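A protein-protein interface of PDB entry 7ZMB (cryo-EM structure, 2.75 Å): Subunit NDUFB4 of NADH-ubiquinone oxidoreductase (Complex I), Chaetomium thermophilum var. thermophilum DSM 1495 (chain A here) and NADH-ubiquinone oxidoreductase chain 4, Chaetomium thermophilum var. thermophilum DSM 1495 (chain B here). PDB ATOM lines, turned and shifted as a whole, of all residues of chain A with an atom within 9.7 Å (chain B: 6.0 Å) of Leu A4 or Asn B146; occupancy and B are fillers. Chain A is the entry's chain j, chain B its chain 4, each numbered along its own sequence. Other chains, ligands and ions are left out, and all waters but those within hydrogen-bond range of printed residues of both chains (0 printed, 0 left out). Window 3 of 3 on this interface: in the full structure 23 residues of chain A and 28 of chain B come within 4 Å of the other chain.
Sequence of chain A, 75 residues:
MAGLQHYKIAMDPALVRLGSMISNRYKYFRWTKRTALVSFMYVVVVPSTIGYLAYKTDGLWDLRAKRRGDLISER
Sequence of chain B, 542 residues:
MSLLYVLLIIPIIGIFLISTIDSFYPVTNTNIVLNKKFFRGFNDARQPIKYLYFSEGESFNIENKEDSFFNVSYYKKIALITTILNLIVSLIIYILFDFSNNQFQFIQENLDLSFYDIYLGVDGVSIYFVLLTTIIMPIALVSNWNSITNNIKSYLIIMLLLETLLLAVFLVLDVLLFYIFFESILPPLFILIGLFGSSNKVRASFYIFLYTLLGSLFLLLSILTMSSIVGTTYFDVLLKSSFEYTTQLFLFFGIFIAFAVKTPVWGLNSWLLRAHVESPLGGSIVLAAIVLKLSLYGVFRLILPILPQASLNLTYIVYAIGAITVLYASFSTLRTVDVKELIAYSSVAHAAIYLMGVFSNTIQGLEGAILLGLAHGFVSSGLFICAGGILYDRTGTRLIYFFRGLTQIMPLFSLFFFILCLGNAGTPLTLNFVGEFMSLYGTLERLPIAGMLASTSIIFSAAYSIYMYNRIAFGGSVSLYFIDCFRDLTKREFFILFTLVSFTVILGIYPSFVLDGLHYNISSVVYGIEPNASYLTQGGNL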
ATOM      1  N   GLY A   3      18.823   0.432   2.558  1.00  0.00           N
ATOM      2  CA  GLY A   3      17.929   1.539   2.276  1.00  0.00           C
ATOM      3  C   GLY A   3      16.529   1.324   2.812  1.00  0.00           C
ATOM      4  O   GLY A   3      15.810   2.281   3.098  1.00  0.00           O
ATOM      5  N   LEU A   4      16.141   0.059   2.946  1.00  0.00           N
ATOM      6  CA  LEU A   4      14.828  -0.274   3.470  1.00  0.00           C
ATOM      7  C   LEU A   4      14.787  -0.058   4.981  1.00  0.00           C
ATOM      8  O   LEU A   4      15.814   0.075   5.650  1.00  0.00           O
ATOM      9  CB  LEU A   4      14.464  -1.716   3.112  1.00  0.00           C
ATOM     10  CG  LEU A   4      15.374  -2.853   3.591  1.00  0.00           C
ATOM     11  CD1 LEU A   4      15.025  -3.329   4.996  1.00  0.00           C
ATOM     12  CD2 LEU A   4      15.342  -4.012   2.603  1.00  0.00           C
ATOM     13  N   GLN A   5      13.573  -0.023   5.518  1.00  0.00           N
ATOM     14  CA  GLN A   5      13.364   0.133   6.949  1.00  0.00           C
ATOM     15  C   GLN A   5      13.194  -1.231   7.603  1.00  0.00           C
ATOM     16  O   GLN A   5      12.676  -2.173   6.998  1.00  0.00           O
ATOM     17  CB  GLN A   5      12.149   1.019   7.240  1.00  0.00           C
ATOM     18  CG  GLN A   5      10.815   0.419   6.843  1.00  0.00           C
ATOM     19  CD  GLN A   5       9.646   1.211   7.389  1.00  0.00           C
ATOM     20  OE1 GLN A   5       9.513   1.387   8.600  1.00  0.00           O
ATOM     21  NE2 GLN A   5       8.790   1.693   6.497  1.00  0.00           N
ATOM     22  N   HIS A   6      13.651  -1.325   8.851  1.00  0.00           N
ATOM     23  CA  HIS A   6      13.702  -2.558   9.616  1.00  0.00           C
ATOM     24  C   HIS A   6      12.690  -2.503  10.756  1.00  0.00           C
ATOM     25  O   HIS A   6      11.886  -1.575  10.858  1.00  0.00           O
ATOM     26  CB  HIS A   6      15.119  -2.792  10.139  1.00  0.00           C
ATOM     27  CG  HIS A   6      15.688  -1.628  10.885  1.00  0.00           C
ATOM     28  ND1 HIS A   6      15.699  -1.559  12.260  1.00  0.00           N
ATOM     29  CD2 HIS A   6      16.261  -0.483  10.448  1.00  0.00           C
ATOM     30  CE1 HIS A   6      16.257  -0.425  12.637  1.00  0.00           C
ATOM     31  NE2 HIS A   6      16.605   0.248  11.556  1.00  0.00           N
ATOM     32  N   TYR A   7      12.727  -3.518  11.616  1.00  0.00           N
ATOM     33  CA  TYR A   7      11.846  -3.550  12.770  1.00  0.00           C
ATOM     34  C   TYR A   7      12.306  -2.554  13.824  1.00  0.00           C
ATOM     35  O   TYR A   7      13.424  -2.038  13.789  1.00  0.00           O
ATOM     36  CB  TYR A   7      11.783  -4.950  13.377  1.00  0.00           C
ATOM     37  CG  TYR A   7      10.967  -5.921  12.569  1.00  0.00           C
ATOM     38  CD1 TYR A   7       9.650  -5.648  12.262  1.00  0.00           C
ATOM     39  CD2 TYR A   7      11.518  -7.103  12.102  1.00  0.00           C
ATOM     40  CE1 TYR A   7       8.898  -6.517  11.516  1.00  0.00           C
ATOM     41  CE2 TYR A   7      10.772  -7.991  11.363  1.00  0.00           C
ATOM     42  CZ  TYR A   7       9.460  -7.689  11.066  1.00  0.00           C
ATOM     43  OH  TYR A   7       8.701  -8.559  10.321  1.00  0.00           O
ATOM     44  N   LYS B  76      16.753  -7.268 -12.348  1.00  0.00           N
ATOM     45  CA  LYS B  76      17.117  -8.400 -11.508  1.00  0.00           C
ATOM     46  C   LYS B  76      16.710  -9.718 -12.150  1.00  0.00           C
ATOM     47  O   LYS B  76      17.409 -10.723 -11.998  1.00  0.00           O
ATOM     48  CB  LYS B  76      16.475  -8.244 -10.136  1.00  0.00           C
ATOM     49  CG  LYS B  76      16.450  -6.821  -9.675  1.00  0.00           C
ATOM     50  CD  LYS B  76      15.329  -6.564  -8.713  1.00  0.00           C
ATOM     51  CE  LYS B  76      15.574  -7.244  -7.400  1.00  0.00           C
ATOM     52  NZ  LYS B  76      14.624  -6.758  -6.375  1.00  0.00           N
ATOM     53  N   VAL B 142      20.090 -13.393  -5.394  1.00  0.00           N
ATOM     54  CA  VAL B 142      18.846 -13.595  -4.669  1.00  0.00           C
ATOM     55  C   VAL B 142      18.958 -13.095  -3.237  1.00  0.00           C
ATOM     56  O   VAL B 142      17.997 -12.543  -2.704  1.00  0.00           O
ATOM     57  CB  VAL B 142      18.450 -15.081  -4.742  1.00  0.00           C
ATOM     58  CG1 VAL B 142      17.284 -15.370  -3.852  1.00  0.00           C
ATOM     59  CG2 VAL B 142      18.114 -15.467  -6.173  1.00  0.00           C
ATOM     60  N   SER B 143      20.132 -13.223  -2.618  1.00  0.00           N
ATOM     61  CA  SER B 143      20.329 -12.753  -1.252  1.00  0.00           C
ATOM     62  C   SER B 143      20.141 -11.245  -1.101  1.00  0.00           C
ATOM     63  O   SER B 143      19.800 -10.784  -0.007  1.00  0.00           O
ATOM     64  CB  SER B 143      21.718 -13.164  -0.765  1.00  0.00           C
ATOM     65  OG  SER B 143      22.741 -12.524  -1.507  1.00  0.00           O
ATOM     66  N   ASN B 144      20.366 -10.459  -2.152  1.00  0.00           N
ATOM     67  CA  ASN B 144      20.094  -9.023  -2.132  1.00  0.00           C
ATOM     68  C   ASN B 144      18.931  -8.631  -3.031  1.00  0.00           C
ATOM     69  O   ASN B 144      18.906  -7.519  -3.559  1.00  0.00           O
ATOM     70  CB  ASN B 144      21.323  -8.196  -2.515  1.00  0.00           C
ATOM     71  CG  ASN B 144      22.420  -8.274  -1.499  1.00  0.00           C
ATOM     72  OD1 ASN B 144      23.490  -8.801  -1.763  1.00  0.00           O
ATOM     73  ND2 ASN B 144      22.174  -7.713  -0.332  1.00  0.00           N
ATOM     74  N   TRP B 145      17.956  -9.523  -3.200  1.00  0.00           N
ATOM     75  CA  TRP B 145      16.828  -9.206  -4.062  1.00  0.00           C
ATOM     76  C   TRP B 145      16.057  -7.993  -3.559  1.00  0.00           C
ATOM     77  O   TRP B 145      15.602  -7.172  -4.360  1.00  0.00           O
ATOM     78  CB  TRP B 145      15.911 -10.415  -4.190  1.00  0.00           C
ATOM     79  CG  TRP B 145      14.917 -10.298  -5.306  1.00  0.00           C
ATOM     80  CD1 TRP B 145      13.673  -9.761  -5.233  1.00  0.00           C
ATOM     81  CD2 TRP B 145      15.092 -10.722  -6.661  1.00  0.00           C
ATOM     82  NE1 TRP B 145      13.056  -9.828  -6.451  1.00  0.00           N
ATOM     83  CE2 TRP B 145      13.906 -10.412  -7.348  1.00  0.00           C
ATOM     84  CE3 TRP B 145      16.136 -11.336  -7.361  1.00  0.00           C
ATOM     85  CZ2 TRP B 145      13.733 -10.693  -8.697  1.00  0.00           C
ATOM     86  CZ3 TRP B 145      15.961 -11.617  -8.695  1.00  0.00           C
ATOM     87  CH2 TRP B 145      14.770 -11.299  -9.351  1.00  0.00           C
ATOM     88  N   ASN B 146      15.910  -7.844  -2.249  1.00  0.00           N
ATOM     89  CA  ASN B 146      15.240  -6.682  -1.707  1.00  0.00           C
ATOM     90  C   ASN B 146      16.177  -5.684  -1.053  1.00  0.00           C
ATOM     91  O   ASN B 146      15.819  -4.509  -0.946  1.00  0.00           O
ATOM     92  CB  ASN B 146      14.174  -7.109  -0.689  1.00  0.00           C
ATOM     93  CG  ASN B 146      13.054  -7.903  -1.318  1.00  0.00           C
ATOM     94  OD1 ASN B 146      12.712  -8.977  -0.848  1.00  0.00           O
ATOM     95  ND2 ASN B 146      12.481  -7.380  -2.392  1.00  0.00           N
ATOM     96  N   SER B 147      17.368  -6.103  -0.637  1.00  0.00           N
ATOM     97  CA  SER B 147      18.230  -5.238   0.154  1.00  0.00           C
ATOM     98  C   SER B 147      18.835  -4.112  -0.671  1.00  0.00           C
ATOM     99  O   SER B 147      19.090  -3.029  -0.137  1.00  0.00           O
ATOM    100  CB  SER B 147      19.327  -6.071   0.800  1.00  0.00           C
ATOM    101  OG  SER B 147      18.769  -6.998   1.707  1.00  0.00           O
ATOM    102  N   ILE B 148      19.078  -4.344  -1.955  1.00  0.00           N
ATOM    103  CA  ILE B 148      19.578  -3.295  -2.832  1.00  0.00           C
ATOM    104  C   ILE B 148      18.393  -2.459  -3.283  1.00  0.00           C
ATOM    105  O   ILE B 148      17.452  -2.978  -3.891  1.00  0.00           O
ATOM    106  CB  ILE B 148      20.334  -3.877  -4.036  1.00  0.00           C
ATOM    107  CG1 ILE B 148      21.538  -4.705  -3.585  1.00  0.00           C
ATOM    108  CG2 ILE B 148      20.765  -2.768  -4.977  1.00  0.00           C
ATOM    109  CD1 ILE B 148      22.582  -3.914  -2.867  1.00  0.00           C
ATOM    110  N   THR B 149      18.436  -1.166  -2.995  1.00  0.00           N
ATOM    111  CA  THR B 149      17.381  -0.251  -3.399  1.00  0.00           C
ATOM    112  C   THR B 149      17.821   0.731  -4.470  1.00  0.00           C
ATOM    113  O   THR B 149      17.214   0.780  -5.540  1.00  0.00           O
ATOM    114  CB  THR B 149      16.864   0.524  -2.186  1.00  0.00           C
ATOM    115  OG1 THR B 149      17.915   1.344  -1.659  1.00  0.00           O
ATOM    116  CG2 THR B 149      16.405  -0.442  -1.110  1.00  0.00           C
ATOM    117  N   ASP B 393      18.906  -7.265   8.316  1.00  0.00           N
ATOM    118  CA  ASP B 393      17.740  -6.726   7.627  1.00  0.00           C
ATOM    119  C   ASP B 393      16.621  -6.405   8.607  1.00  0.00           C
ATOM    120  O   ASP B 393      15.978  -5.356   8.501  1.00  0.00           O
ATOM    121  CB  ASP B 393      17.254  -7.710   6.570  1.00  0.00           C
ATOM    122  CG  ASP B 393      18.033  -7.610   5.282  1.00  0.00           C
ATOM    123  OD1 ASP B 393      19.181  -7.134   5.321  1.00  0.00           O
ATOM    124  OD2 ASP B 393      17.497  -8.009   4.227  1.00  0.00           O
ATOM    125  N   ARG B 492      12.247 -16.645   0.204  1.00  0.00           N
ATOM    126  CA  ARG B 492      13.563 -16.378  -0.367  1.00  0.00           C
ATOM    127  C   ARG B 492      14.662 -16.863   0.561  1.00  0.00           C
ATOM    128  O   ARG B 492      15.587 -17.567   0.140  1.00  0.00           O
ATOM    129  CB  ARG B 492      13.759 -14.890  -0.624  1.00  0.00           C
ATOM    130  CG  ARG B 492      15.053 -14.643  -1.335  1.00  0.00           C
ATOM    131  CD  ARG B 492      15.312 -13.206  -1.678  1.00  0.00           C
ATOM    132  NE  ARG B 492      15.480 -12.385  -0.491  1.00  0.00           N
ATOM    133  CZ  ARG B 492      14.642 -11.434  -0.123  1.00  0.00           C
ATOM    134  NH1 ARG B 492      14.874 -10.740   0.978  1.00  0.00           N
ATOM    135  NH2 ARG B 492      13.562 -11.189  -0.851  1.00  0.00           N
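The side-chain amide oxygen of Asn B146 lies close to the guanidinium group of Arg B492, 3.3 Å away.
OG of Ser B147 lies within hydrogen-bond range of OD2 of Asp B393 (3.0 Å).
Thr B149 touches Gly A3.
CD2 of Leu A4 touches O of Asn B146 (3.6 Å).
Leu A4 touches Ser B147 (CD2 to CA, 3.98 Å).
His A6 touches Asp B393 (CB to O, 3.2 Å).
Of the printed residues of chain A, Asp B393 touches His A6.
Of the printed residues of chain B, His A6 touches Asp B393.
Of the printed residues of chain A, Ser B147 touches Leu A4 (3.98 Å).
Val B142 touches none of the printed residues of chain A.
Tyr A7 touches none of the printed residues of chain B.
The nearest printed residue of chain B that does not touch Leu A4 is Thr B149 (4.1 Å).
The nearest residue of chain A that does not touch Asn B146 is Gly A3 (6.8 Å).
The nearest printed residue of chain B that does not touch His A6 is Ser B147 (10.1 Å).
Hydrophobic or aromatic side chains of chain A within 4 Å of the printed part of chain B: Leu A4 and His A6.
Along chain A the printed residues that touch a printed residue of chain B span positions 3 to 6.
Among the printed residues, no Asp or Glu carboxylate lies within 4 Å of a Lys or Arg side-chain nitrogen of the other chain.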
